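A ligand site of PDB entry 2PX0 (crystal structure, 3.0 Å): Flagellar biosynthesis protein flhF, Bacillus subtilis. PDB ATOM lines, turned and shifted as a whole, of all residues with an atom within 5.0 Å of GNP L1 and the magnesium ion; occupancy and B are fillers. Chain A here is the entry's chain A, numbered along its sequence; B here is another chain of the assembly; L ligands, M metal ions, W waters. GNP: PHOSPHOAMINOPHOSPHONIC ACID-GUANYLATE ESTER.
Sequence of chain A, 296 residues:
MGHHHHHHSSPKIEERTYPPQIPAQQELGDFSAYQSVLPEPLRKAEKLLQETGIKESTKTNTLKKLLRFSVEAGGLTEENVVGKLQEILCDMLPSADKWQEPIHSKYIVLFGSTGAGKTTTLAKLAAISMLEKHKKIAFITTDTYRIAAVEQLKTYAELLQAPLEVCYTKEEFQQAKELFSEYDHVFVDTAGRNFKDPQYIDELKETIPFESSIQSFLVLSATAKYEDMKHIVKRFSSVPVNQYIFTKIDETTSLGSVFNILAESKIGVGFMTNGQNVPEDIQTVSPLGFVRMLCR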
ATOM      1  N   SER A 113     -11.273  -6.658 -26.577  1.00  0.00           N
ATOM      2  CA  SER A 113     -10.070  -7.199 -27.197  1.00  0.00           C
ATOM      3  C   SER A 113      -8.947  -7.506 -26.214  1.00  0.00           C
ATOM      4  O   SER A 113      -8.935  -7.021 -25.079  1.00  0.00           O
ATOM      5  CB  SER A 113      -9.599  -6.189 -28.230  1.00  0.00           C
ATOM      6  OG  SER A 113     -10.686  -5.360 -28.610  1.00  0.00           O
ATOM      7  N   THR A 114      -7.988  -8.313 -26.656  1.00  0.00           N
ATOM      8  CA  THR A 114      -6.873  -8.678 -25.816  1.00  0.00           C
ATOM      9  C   THR A 114      -5.924  -7.490 -25.607  1.00  0.00           C
ATOM     10  O   THR A 114      -5.728  -6.680 -26.513  1.00  0.00           O
ATOM     11  CB  THR A 114      -6.068  -9.862 -26.414  1.00  0.00           C
ATOM     12  OG1 THR A 114      -5.830  -9.638 -27.802  1.00  0.00           O
ATOM     13  CG2 THR A 114      -6.825 -11.154 -26.239  1.00  0.00           C
ATOM     14  N   GLY A 115      -5.379  -7.395 -24.397  1.00  0.00           N
ATOM     15  CA  GLY A 115      -4.448  -6.340 -24.040  1.00  0.00           C
ATOM     16  C   GLY A 115      -4.906  -4.922 -24.280  1.00  0.00           C
ATOM     17  O   GLY A 115      -4.096  -3.999 -24.222  1.00  0.00           O
ATOM     18  N   ALA A 116      -6.188  -4.719 -24.534  1.00  0.00           N
ATOM     19  CA  ALA A 116      -6.692  -3.386 -24.802  1.00  0.00           C
ATOM     20  C   ALA A 116      -6.535  -2.447 -23.608  1.00  0.00           C
ATOM     21  O   ALA A 116      -6.193  -1.269 -23.777  1.00  0.00           O
ATOM     22  CB  ALA A 116      -8.144  -3.443 -25.235  1.00  0.00           C
ATOM     23  N   GLY A 117      -6.789  -2.962 -22.410  1.00  0.00           N
ATOM     24  CA  GLY A 117      -6.674  -2.158 -21.213  1.00  0.00           C
ATOM     25  C   GLY A 117      -7.932  -2.235 -20.380  1.00  0.00           C
ATOM     26  O   GLY A 117      -8.386  -1.236 -19.839  1.00  0.00           O
ATOM     27  N   LYS A 118      -8.504  -3.412 -20.258  1.00  0.00           N
ATOM     28  CA  LYS A 118      -9.720  -3.551 -19.484  1.00  0.00           C
ATOM     29  C   LYS A 118      -9.472  -3.400 -17.995  1.00  0.00           C
ATOM     30  O   LYS A 118     -10.087  -2.569 -17.330  1.00  0.00           O
ATOM     31  CB  LYS A 118     -10.389  -4.899 -19.739  1.00  0.00           C
ATOM     32  CG  LYS A 118     -11.033  -5.011 -21.095  1.00  0.00           C
ATOM     33  CD  LYS A 118     -11.725  -6.343 -21.220  1.00  0.00           C
ATOM     34  CE  LYS A 118     -10.700  -7.453 -21.264  1.00  0.00           C
ATOM     35  NZ  LYS A 118      -9.686  -7.260 -22.328  1.00  0.00           N
ATOM     36  N   THR A 119      -8.577  -4.220 -17.473  1.00  0.00           N
ATOM     37  CA  THR A 119      -8.277  -4.207 -16.058  1.00  0.00           C
ATOM     38  C   THR A 119      -7.714  -2.875 -15.531  1.00  0.00           C
ATOM     39  O   THR A 119      -8.155  -2.365 -14.493  1.00  0.00           O
ATOM     40  CB  THR A 119      -7.311  -5.327 -15.713  1.00  0.00           C
ATOM     41  OG1 THR A 119      -7.730  -6.519 -16.382  1.00  0.00           O
ATOM     42  CG2 THR A 119      -7.301  -5.571 -14.212  1.00  0.00           C
ATOM     43  N   THR A 120      -6.735  -2.309 -16.234  1.00  0.00           N
ATOM     44  CA  THR A 120      -6.171  -1.057 -15.789  1.00  0.00           C
ATOM     45  C   THR A 120      -7.257  -0.022 -15.788  1.00  0.00           C
ATOM     46  O   THR A 120      -7.249   0.913 -14.988  1.00  0.00           O
ATOM     47  CB  THR A 120      -5.073  -0.575 -16.726  1.00  0.00           C
ATOM     48  OG1 THR A 120      -4.116  -1.626 -16.919  1.00  0.00           O
ATOM     49  CG2 THR A 120      -4.393   0.649 -16.123  1.00  0.00           C
ATOM     50  N   THR A 121      -8.204  -0.194 -16.706  1.00  0.00           N
ATOM     51  CA  THR A 121      -9.297   0.731 -16.846  1.00  0.00           C
ATOM     52  C   THR A 121     -10.345   0.490 -15.787  1.00  0.00           C
ATOM     53  O   THR A 121     -10.866   1.416 -15.188  1.00  0.00           O
ATOM     54  CB  THR A 121      -9.932   0.639 -18.236  1.00  0.00           C
ATOM     55  OG1 THR A 121      -8.926   0.895 -19.220  1.00  0.00           O
ATOM     56  CG2 THR A 121     -11.045   1.675 -18.393  1.00  0.00           C
ATOM     57  N   LYS A 124      -8.792   2.094 -12.943  1.00  0.00           N
ATOM     58  CA  LYS A 124      -8.895   3.539 -12.866  1.00  0.00           C
ATOM     59  C   LYS A 124     -10.326   3.886 -12.461  1.00  0.00           C
ATOM     60  O   LYS A 124     -10.558   4.655 -11.526  1.00  0.00           O
ATOM     61  CB  LYS A 124      -8.582   4.167 -14.221  1.00  0.00           C
ATOM     62  CG  LYS A 124      -7.152   3.974 -14.681  1.00  0.00           C
ATOM     63  CD  LYS A 124      -6.884   4.629 -16.025  1.00  0.00           C
ATOM     64  CE  LYS A 124      -5.439   4.432 -16.422  1.00  0.00           C
ATOM     65  NZ  LYS A 124      -5.190   4.735 -17.851  1.00  0.00           N
ATOM     66  N   ASP A 143     -12.187 -13.450 -15.137  1.00  0.00           N
ATOM     67  CA  ASP A 143     -10.972 -13.843 -15.809  1.00  0.00           C
ATOM     68  C   ASP A 143     -10.286 -15.001 -15.124  1.00  0.00           C
ATOM     69  O   ASP A 143      -9.357 -14.825 -14.329  1.00  0.00           O
ATOM     70  CB  ASP A 143      -9.995 -12.669 -15.928  1.00  0.00           C
ATOM     71  CG  ASP A 143      -8.810 -13.022 -16.786  1.00  0.00           C
ATOM     72  OD1 ASP A 143      -8.109 -13.997 -16.454  1.00  0.00           O
ATOM     73  OD2 ASP A 143      -8.562 -12.327 -17.789  1.00  0.00           O
ATOM     74  N   ARG A 146      -6.639 -16.098 -18.138  1.00  0.00           N
ATOM     75  CA  ARG A 146      -5.308 -15.512 -17.996  1.00  0.00           C
ATOM     76  C   ARG A 146      -4.578 -15.869 -16.708  1.00  0.00           C
ATOM     77  O   ARG A 146      -5.079 -15.655 -15.601  1.00  0.00           O
ATOM     78  CB  ARG A 146      -5.380 -13.991 -18.124  1.00  0.00           C
ATOM     79  CG  ARG A 146      -4.049 -13.310 -17.842  1.00  0.00           C
ATOM     80  CD  ARG A 146      -4.058 -11.844 -18.183  1.00  0.00           C
ATOM     81  NE  ARG A 146      -2.834 -11.207 -17.712  1.00  0.00           N
ATOM     82  CZ  ARG A 146      -2.334 -10.090 -18.218  1.00  0.00           C
ATOM     83  NH1 ARG A 146      -2.940  -9.474 -19.223  1.00  0.00           N
ATOM     84  NH2 ARG A 146      -1.207  -9.583 -17.728  1.00  0.00           N
ATOM     85  N   ASP A 189     -14.533  -7.483 -14.045  1.00  0.00           N
ATOM     86  CA  ASP A 189     -13.478  -7.573 -15.053  1.00  0.00           C
ATOM     87  C   ASP A 189     -13.734  -8.896 -15.784  1.00  0.00           C
ATOM     88  O   ASP A 189     -14.324  -9.812 -15.201  1.00  0.00           O
ATOM     89  CB  ASP A 189     -12.107  -7.566 -14.349  1.00  0.00           C
ATOM     90  CG  ASP A 189     -10.912  -7.556 -15.304  1.00  0.00           C
ATOM     91  OD1 ASP A 189     -11.077  -7.197 -16.493  1.00  0.00           O
ATOM     92  OD2 ASP A 189      -9.781  -7.887 -14.859  1.00  0.00           O
ATOM     93  N   THR A 190     -13.348  -8.987 -17.054  1.00  0.00           N
ATOM     94  CA  THR A 190     -13.579 -10.204 -17.838  1.00  0.00           C
ATOM     95  C   THR A 190     -12.329 -10.664 -18.590  1.00  0.00           C
ATOM     96  O   THR A 190     -11.387  -9.900 -18.753  1.00  0.00           O
ATOM     97  CB  THR A 190     -14.717 -10.014 -18.872  1.00  0.00           C
ATOM     98  OG1 THR A 190     -14.262  -9.150 -19.926  1.00  0.00           O
ATOM     99  CG2 THR A 190     -15.944  -9.401 -18.219  1.00  0.00           C
ATOM    100  N   ALA A 191     -12.348 -11.908 -19.042  1.00  0.00           N
ATOM    101  CA  ALA A 191     -11.224 -12.493 -19.774  1.00  0.00           C
ATOM    102  C   ALA A 191     -11.072 -11.949 -21.195  1.00  0.00           C
ATOM    103  O   ALA A 191     -12.055 -11.659 -21.894  1.00  0.00           O
ATOM    104  CB  ALA A 191     -11.366 -13.983 -19.817  1.00  0.00           C
ATOM    105  N   GLY A 192      -9.837 -11.824 -21.624  1.00  0.00           N
ATOM    106  CA  GLY A 192      -9.597 -11.322 -22.958  1.00  0.00           C
ATOM    107  C   GLY A 192      -9.427 -12.444 -23.960  1.00  0.00           C
ATOM    108  O   GLY A 192      -8.306 -12.862 -24.260  1.00  0.00           O
ATOM    109  N   THR A 247      -9.045   3.000 -25.562  1.00  0.00           N
ATOM    110  CA  THR A 247      -7.816   3.192 -24.823  1.00  0.00           C
ATOM    111  C   THR A 247      -6.643   3.613 -25.683  1.00  0.00           C
ATOM    112  O   THR A 247      -6.716   3.625 -26.915  1.00  0.00           O
ATOM    113  CB  THR A 247      -7.439   1.907 -24.111  1.00  0.00           C
ATOM    114  OG1 THR A 247      -7.114   0.924 -25.091  1.00  0.00           O
ATOM    115  CG2 THR A 247      -8.598   1.397 -23.234  1.00  0.00           C
ATOM    116  N   LYS A 248      -5.560   3.975 -25.027  1.00  0.00           N
ATOM    117  CA  LYS A 248      -4.318   4.351 -25.682  1.00  0.00           C
ATOM    118  C   LYS A 248      -4.392   5.447 -26.743  1.00  0.00           C
ATOM    119  O   LYS A 248      -3.602   5.437 -27.708  1.00  0.00           O
ATOM    120  CB  LYS A 248      -3.705   3.083 -26.278  1.00  0.00           C
ATOM    121  CG  LYS A 248      -3.977   1.860 -25.414  1.00  0.00           C
ATOM    122  CD  LYS A 248      -3.156   0.667 -25.823  1.00  0.00           C
ATOM    123  CE  LYS A 248      -3.324  -0.449 -24.805  1.00  0.00           C
ATOM    124  NZ  LYS A 248      -2.439  -1.608 -25.046  1.00  0.00           N
ATOM    125  N   ASP A 250      -3.333   8.138 -26.426  1.00  0.00           N
ATOM    126  CA  ASP A 250      -2.048   8.799 -26.319  1.00  0.00           C
ATOM    127  C   ASP A 250      -1.001   7.950 -26.992  1.00  0.00           C
ATOM    128  O   ASP A 250       0.186   8.271 -26.947  1.00  0.00           O
ATOM    129  CB  ASP A 250      -1.656   8.930 -24.850  1.00  0.00           C
ATOM    130  CG  ASP A 250      -1.283   7.583 -24.236  1.00  0.00           C
ATOM    131  OD1 ASP A 250      -2.157   6.696 -24.185  1.00  0.00           O
ATOM    132  OD2 ASP A 250      -0.113   7.414 -23.801  1.00  0.00           O
ATOM    133  N   GLU A 251      -1.414   6.849 -27.622  1.00  0.00           N
ATOM    134  CA  GLU A 251      -0.467   5.950 -28.253  1.00  0.00           C
ATOM    135  C   GLU A 251      -0.663   5.835 -29.768  1.00  0.00           C
ATOM    136  O   GLU A 251       0.208   5.310 -30.480  1.00  0.00           O
ATOM    137  CB  GLU A 251      -0.584   4.570 -27.608  1.00  0.00           C
ATOM    138  CG  GLU A 251       0.618   3.675 -27.796  1.00  0.00           C
ATOM    139  CD  GLU A 251       0.589   2.510 -26.827  1.00  0.00           C
ATOM    140  OE1 GLU A 251       0.211   2.716 -25.655  1.00  0.00           O
ATOM    141  OE2 GLU A 251       0.935   1.382 -27.225  1.00  0.00           O
ATOM    142  N   THR A 273      -8.847   6.553 -22.473  1.00  0.00           N
ATOM    143  CA  THR A 273      -7.701   6.535 -21.574  1.00  0.00           C
ATOM    144  C   THR A 273      -6.513   7.148 -22.287  1.00  0.00           C
ATOM    145  O   THR A 273      -6.443   7.098 -23.504  1.00  0.00           O
ATOM    146  CB  THR A 273      -7.399   5.105 -21.147  1.00  0.00           C
ATOM    147  OG1 THR A 273      -7.145   4.325 -22.310  1.00  0.00           O
ATOM    148  CG2 THR A 273      -8.586   4.501 -20.425  1.00  0.00           C
ATOM    149  N   ASN A 274      -5.579   7.748 -21.527  1.00  0.00           N
ATOM    150  CA  ASN A 274      -4.412   8.397 -22.149  1.00  0.00           C
ATOM    151  C   ASN A 274      -3.068   8.100 -21.506  1.00  0.00           C
ATOM    152  O   ASN A 274      -2.137   8.893 -21.635  1.00  0.00           O
ATOM    153  CB  ASN A 274      -4.612   9.919 -22.191  1.00  0.00           C
ATOM    154  CG  ASN A 274      -5.064  10.491 -20.847  1.00  0.00           C
ATOM    155  OD1 ASN A 274      -6.188  10.251 -20.395  1.00  0.00           O
ATOM    156  ND2 ASN A 274      -4.193  11.250 -20.216  1.00  0.00           N
ATOM    157  N   GLY A 275      -2.951   6.953 -20.840  1.00  0.00           N
ATOM    158  CA  GLY A 275      -1.696   6.586 -20.209  1.00  0.00           C
ATOM    159  C   GLY A 275      -1.855   5.430 -19.235  1.00  0.00           C
ATOM    160  O   GLY A 275      -2.918   4.840 -19.152  1.00  0.00           O
ATOM    161  N   GLN A 276      -0.805   5.124 -18.482  1.00  0.00           N
ATOM    162  CA  GLN A 276      -0.862   4.006 -17.546  1.00  0.00           C
ATOM    163  C   GLN A 276      -1.044   4.410 -16.074  1.00  0.00           C
ATOM    164  O   GLN A 276      -1.294   3.550 -15.229  1.00  0.00           O
ATOM    165  CB  GLN A 276       0.410   3.163 -17.707  1.00  0.00           C
ATOM    166  CG  GLN A 276       1.093   3.406 -19.021  1.00  0.00           C
ATOM    167  CD  GLN A 276       2.228   2.429 -19.305  1.00  0.00           C
ATOM    168  OE1 GLN A 276       2.000   1.231 -19.435  1.00  0.00           O
ATOM    169  NE2 GLN A 276       3.447   2.948 -19.418  1.00  0.00           N
ATOM    170  N   ASP A 281      -4.704   8.901 -15.609  1.00  0.00           N
ATOM    171  CA  ASP A 281      -4.893   8.699 -17.036  1.00  0.00           C
ATOM    172  C   ASP A 281      -6.210   8.103 -17.540  1.00  0.00           C
ATOM    173  O   ASP A 281      -6.265   6.979 -18.025  1.00  0.00           O
ATOM    174  CB  ASP A 281      -3.704   7.895 -17.559  1.00  0.00           C
ATOM    175  CG  ASP A 281      -2.382   8.619 -17.361  1.00  0.00           C
ATOM    176  OD1 ASP A 281      -2.434   9.789 -16.942  1.00  0.00           O
ATOM    177  OD2 ASP A 281      -1.307   8.027 -17.607  1.00  0.00           O
ATOM    178  N   THR B 114       2.340  -2.126 -25.597  1.00  0.00           N
ATOM    179  CA  THR B 114       1.572  -2.564 -24.444  1.00  0.00           C
ATOM    180  C   THR B 114       0.413  -3.495 -24.740  1.00  0.00           C
ATOM    181  O   THR B 114      -0.591  -3.095 -25.312  1.00  0.00           O
ATOM    182  CB  THR B 114       1.036  -1.342 -23.684  1.00  0.00           C
ATOM    183  OG1 THR B 114       0.212  -0.561 -24.559  1.00  0.00           O
ATOM    184  CG2 THR B 114       2.172  -0.499 -23.203  1.00  0.00           C
ATOM    185  N   GLY B 115       0.546  -4.753 -24.320  1.00  0.00           N
ATOM    186  CA  GLY B 115      -0.508  -5.735 -24.514  1.00  0.00           C
ATOM    187  C   GLY B 115      -0.398  -6.599 -25.746  1.00  0.00           C
ATOM    188  O   GLY B 115      -1.296  -7.404 -25.998  1.00  0.00           O
ATOM    189  N   ARG B 146       4.288  -1.593 -13.258  1.00  0.00           N
ATOM    190  CA  ARG B 146       2.912  -2.030 -13.023  1.00  0.00           C
ATOM    191  C   ARG B 146       2.681  -2.899 -11.785  1.00  0.00           C
ATOM    192  O   ARG B 146       3.457  -3.798 -11.474  1.00  0.00           O
ATOM    193  CB  ARG B 146       2.364  -2.760 -14.249  1.00  0.00           C
ATOM    194  CG  ARG B 146       0.840  -2.859 -14.299  1.00  0.00           C
ATOM    195  CD  ARG B 146       0.392  -4.254 -14.683  1.00  0.00           C
ATOM    196  NE  ARG B 146       0.930  -4.699 -15.969  1.00  0.00           N
ATOM    197  CZ  ARG B 146       1.039  -5.969 -16.339  1.00  0.00           C
ATOM    198  NH1 ARG B 146       0.662  -6.944 -15.524  1.00  0.00           N
ATOM    199  NH2 ARG B 146       1.528  -6.257 -17.532  1.00  0.00           N
ATOM    200  N   GLY B 192       5.870  -2.785 -20.132  1.00  0.00           N
ATOM    201  CA  GLY B 192       5.102  -2.304 -21.263  1.00  0.00           C
ATOM    202  C   GLY B 192       5.081  -0.791 -21.179  1.00  0.00           C
ATOM    203  O   GLY B 192       4.757  -0.224 -20.141  1.00  0.00           O
ATOM    204  N   ASN B 194       4.559   3.140 -23.632  1.00  0.00           N
ATOM    205  CA  ASN B 194       4.253   3.820 -24.885  1.00  0.00           C
ATOM    206  C   ASN B 194       5.591   4.302 -25.422  1.00  0.00           C
ATOM    207  O   ASN B 194       6.083   5.373 -25.032  1.00  0.00           O
ATOM    208  CB  ASN B 194       3.297   4.994 -24.644  1.00  0.00           C
ATOM    209  CG  ASN B 194       3.191   5.920 -25.841  1.00  0.00           C
ATOM    210  OD1 ASN B 194       3.280   5.500 -26.991  1.00  0.00           O
ATOM    211  ND2 ASN B 194       2.975   7.197 -25.570  1.00  0.00           N
HETATM  212  PG  GNP L   1      -6.180  -8.880 -21.019  1.00  0.00           P
HETATM  213  O1G GNP L   1      -4.992  -9.643 -21.491  1.00  0.00           O
HETATM  214  O2G GNP L   1      -6.631  -9.303 -19.610  1.00  0.00           O
HETATM  215  O3G GNP L   1      -7.315  -8.929 -21.984  1.00  0.00           O
HETATM  216  N3B GNP L   1      -5.530  -7.337 -20.908  1.00  0.00           N
HETATM  217  PB  GNP L   1      -6.438  -6.064 -20.380  1.00  0.00           P
HETATM  218  O1B GNP L   1      -7.449  -5.707 -21.355  1.00  0.00           O
HETATM  219  O2B GNP L   1      -6.866  -6.423 -18.989  1.00  0.00           O
HETATM  220  O3A GNP L   1      -5.233  -4.968 -20.405  1.00  0.00           O
HETATM  221  PA  GNP L   1      -4.272  -4.548 -19.263  1.00  0.00           P
HETATM  222  O1A GNP L   1      -5.003  -3.816 -18.189  1.00  0.00           O
HETATM  223  O2A GNP L   1      -3.494  -5.808 -18.932  1.00  0.00           O
HETATM  224  O5' GNP L   1      -3.356  -3.556 -19.938  1.00  0.00           O
HETATM  225  C5' GNP L   1      -2.520  -3.988 -21.024  1.00  0.00           C
HETATM  226  C4' GNP L   1      -1.481  -2.972 -21.331  1.00  0.00           C
HETATM  227  O4' GNP L   1      -1.905  -1.797 -21.934  1.00  0.00           O
HETATM  228  C3' GNP L   1      -0.681  -2.538 -20.069  1.00  0.00           C
HETATM  229  O3' GNP L   1       0.734  -2.576 -20.317  1.00  0.00           O
HETATM  230  C2' GNP L   1      -1.153  -1.116 -19.822  1.00  0.00           C
HETATM  231  O2' GNP L   1      -0.223  -0.292 -19.188  1.00  0.00           O
HETATM  232  C1' GNP L   1      -1.454  -0.669 -21.216  1.00  0.00           C
HETATM  233  N9  GNP L   1      -2.482   0.393 -21.214  1.00  0.00           N
HETATM  234  C8  GNP L   1      -3.846   0.245 -20.736  1.00  0.00           C
HETATM  235  N7  GNP L   1      -4.491   1.373 -20.858  1.00  0.00           N
HETATM  236  C5  GNP L   1      -3.499   2.290 -21.452  1.00  0.00           C
HETATM  237  C6  GNP L   1      -3.638   3.692 -21.823  1.00  0.00           C
HETATM  238  O6  GNP L   1      -4.564   4.392 -21.728  1.00  0.00           O
HETATM  239  N1  GNP L   1      -2.453   4.191 -22.347  1.00  0.00           N
HETATM  240  C2  GNP L   1      -1.351   3.345 -22.452  1.00  0.00           C
HETATM  241  N2  GNP L   1      -0.233   4.029 -23.028  1.00  0.00           N
HETATM  242  N3  GNP L   1      -1.158   2.115 -22.145  1.00  0.00           N
HETATM  243  C4  GNP L   1      -2.329   1.644 -21.632  1.00  0.00           C
HETATM  244  PG  GNP L   2       2.334  -5.839 -20.965  1.00  0.00           P
HETATM  245  O1G GNP L   2       1.219  -5.115 -20.295  1.00  0.00           O
HETATM  246  O2G GNP L   2       3.257  -6.529 -19.939  1.00  0.00           O
HETATM  247  O3G GNP L   2       3.101  -4.974 -21.879  1.00  0.00           O
HETATM  248  N3B GNP L   2       1.471  -7.069 -21.781  1.00  0.00           N
HETATM  249  PB  GNP L   2       2.254  -8.207 -22.685  1.00  0.00           P
HETATM  250  O1B GNP L   2       2.830  -7.642 -23.898  1.00  0.00           O
HETATM  251  O2B GNP L   2       3.144  -8.917 -21.724  1.00  0.00           O
HETATM  252  O3A GNP L   2       1.010  -9.090 -23.105  1.00  0.00           O
HETATM  253  PA  GNP L   2       0.583 -10.413 -22.577  1.00  0.00           P
HETATM  254  O1A GNP L   2       1.586 -11.455 -22.922  1.00  0.00           O
HETATM  255  O2A GNP L   2       0.247 -10.161 -21.124  1.00  0.00           O
HETATM  256  O5' GNP L   2      -0.697 -10.696 -23.366  1.00  0.00           O
HETATM  257  C5' GNP L   2      -1.849  -9.837 -23.223  1.00  0.00           C
HETATM  258  C4' GNP L   2      -3.053 -10.420 -23.895  1.00  0.00           C
HETATM  259  O4' GNP L   2      -2.956 -10.673 -25.258  1.00  0.00           O
HETATM  260  C3' GNP L   2      -3.496 -11.773 -23.243  1.00  0.00           C
HETATM  261  O3' GNP L   2      -4.908 -11.771 -22.938  1.00  0.00           O
HETATM  262  C2' GNP L   2      -3.129 -12.832 -24.307  1.00  0.00           C
HETATM  263  O2' GNP L   2      -3.924 -13.976 -24.286  1.00  0.00           O
HETATM  264  C1' GNP L   2      -3.299 -12.015 -25.564  1.00  0.00           C
HETATM  265  N9  GNP L   2      -2.414 -12.549 -26.637  1.00  0.00           N
HETATM  266  C8  GNP L   2      -0.957 -12.551 -26.583  1.00  0.00           C
HETATM  267  N7  GNP L   2      -0.469 -13.093 -27.679  1.00  0.00           N
HETATM  268  C5  GNP L   2      -1.675 -13.465 -28.473  1.00  0.00           C
HETATM  269  C6  GNP L   2      -1.784 -14.107 -29.786  1.00  0.00           C
HETATM  270  O6  GNP L   2      -0.936 -14.479 -30.495  1.00  0.00           O
HETATM  271  N1  GNP L   2      -3.095 -14.269 -30.171  1.00  0.00           N
HETATM  272  C2  GNP L   2      -4.092 -13.827 -29.329  1.00  0.00           C
HETATM  273  N2  GNP L   2      -5.384 -14.090 -29.921  1.00  0.00           N
HETATM  274  N3  GNP L   2      -4.096 -13.258 -28.174  1.00  0.00           N
HETATM  275  C4  GNP L   2      -2.792 -13.098 -27.795  1.00  0.00           C
HETATM  276 MG    MG M   1      -7.067  -8.183 -17.869  1.00  0.00          MG
HETATM  277  O   HOH W   1      -7.279  -9.928 -16.741  1.00  0.00           O
HETATM  278  O   HOH W   2      -5.034  -8.102 -17.364  1.00  0.00           O
HETATM  279  O   HOH W   3      -9.112  -8.245 -18.320  1.00  0.00           O
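One residue has an atom within 4 Å of the magnesium ion: Thr 119. The nearest printed residue that does not touch the magnesium ion is Asp 189 (4.1 Å).
An oxygen (O1G) of GNP L1 is in hydrogen-bond range of an oxygen (O3') of GNP L2 (2.6 Å).
O1A of GNP L1 lies within hydrogen-bond range of N of Thr 120 (3.0 Å). OG1 of Thr 120 lies within hydrogen-bond range of O1A of GNP L1, 2.7 Å away. The side-chain amino group of Lys 118 is in salt-bridge range of an oxygen (O1B) of GNP L1, 2.9 Å away. The backbone carbonyl oxygen (O) of Gly 275 lies close to a nitrogen (N1) of GNP L1 (3.3 Å). NH2 of Arg 146 of chain B is in salt-bridge range of O1G of GNP L2 (3.0 Å). An oxygen (O3G) of GNP L1 sits at hydrogen-bond distance from the backbone NH (N) of Gly 115 of chain A, at 3.5 Å. The backbone NH (N) of Gly 117 lies within hydrogen-bond range of an oxygen (O1B) of GNP L1, 3.0 Å away. The side-chain carboxylate (OE1) of Glu 251 sits at hydrogen-bond distance from a nitrogen (N2) of GNP L1, 3.0 Å away. N of Lys 248 is in hydrogen-bond range of O6 of GNP L1 (3.5 Å). OG1 of Thr 273 sits at hydrogen-bond distance from O6 of GNP L1, 2.6 Å away. N of Gly 275 is in hydrogen-bond range of O6 of GNP L1 (3.2 Å). The guanidinium group (NH1) of Arg 146 of chain A lies within salt-bridge range of an oxygen (O1G) of GNP L1. OD1 of Asp 250 lies within hydrogen-bond range of N1 of GNP L1 (3.1 Å). An oxygen (O1B) of GNP L1 lies within hydrogen-bond range of the backbone NH of Lys 118, at 2.8 Å. OE1 of Gln 276 lies within hydrogen-bond range of O2' of GNP L1, at 2.7 Å. NH2 of Arg 146 of chain A is in salt-bridge range of O2A of GNP L2, at 3.7 Å. An oxygen (O4') of GNP L1 lies within hydrogen-bond range of the side-chain amino group (NZ) of Lys 248 (3.2 Å). The backbone NH (N) of Thr 119 lies close to an oxygen (O2B) of GNP L1 (3.2 Å).
Ser 113 touches GNP L1 (O to O3G, 3.98 Å). CA of Thr 114 of chain A touches O3G of GNP L1 (3.9 Å). N of Ala 116 touches O1B of GNP L1 (3.6 Å). Lys 124 touches GNP L1 (NZ to O6, 3.9 Å). Gly 192 of chain A touches GNP L1 (CA to O3G, 3.4 Å). Asn 274 touches GNP L1 (N to O6, 3.5 Å). CB of Thr 114 of chain B touches O4' of GNP L1 (3.5 Å). Within 4 Å of GNP L1: Ser 113, Thr 114 of chain A, Gly 115 of chain A, Ala 116, Gly 117, Lys 118, Thr 119, Thr 120, Lys 124, Arg 146 of chain A, Gly 192 of chain A, Lys 248, Asp 250, Glu 251, Thr 273, Asn 274, Gly 275, Gln 276 and Thr 114 of chain B. The nearest printed residue that does not touch GNP L1 is Asn 194 of chain B (4.0004 Å).
The side-chain carboxylate of Asp 189 lies close to the side-chain hydroxyl of Thr 119. The side-chain carboxylate (OE2) of Glu 251 lies within hydrogen-bond range of the side-chain hydroxyl (OG1) of Thr 114 of chain B. ND2 of Asn 194 of chain B is in hydrogen-bond range of O of Asp 250 (3.3 Å). The backbone NH of Arg 146 of chain A is in hydrogen-bond range of the side-chain carboxylate of Asp 143 (3.1 Å). The side-chain amino group of Lys 124 sits at hydrogen-bond distance from the backbone carbonyl oxygen of Asp 281 (2.5 Å). The side-chain amino group of Lys 118 sits at hydrogen-bond distance from the backbone carbonyl oxygen of Ser 113 (2.9 Å). O of Ala 116 is in hydrogen-bond range of OG1 of Thr 247 (2.7 Å). OG1 of Thr 114 of chain B sits at hydrogen-bond distance from NZ of Lys 248.
Water W2 lies within hydrogen-bond range of NH1 of Arg 146 of chain A (3.1 Å) and O2A of GNP L1 (3.2 Å). Water W3 lies within hydrogen-bond range of O of Thr 190 (2.8 Å) and OD1 of Asp 189 (2.9 Å).
The magnesium ion is bound by water W1, water W3, an oxygen (O2B) of GNP L1, water W2, an oxygen (O2G) of GNP L1 and the side-chain hydroxyl of Thr 119. The magnesium ion has six donor atoms within binding distance.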
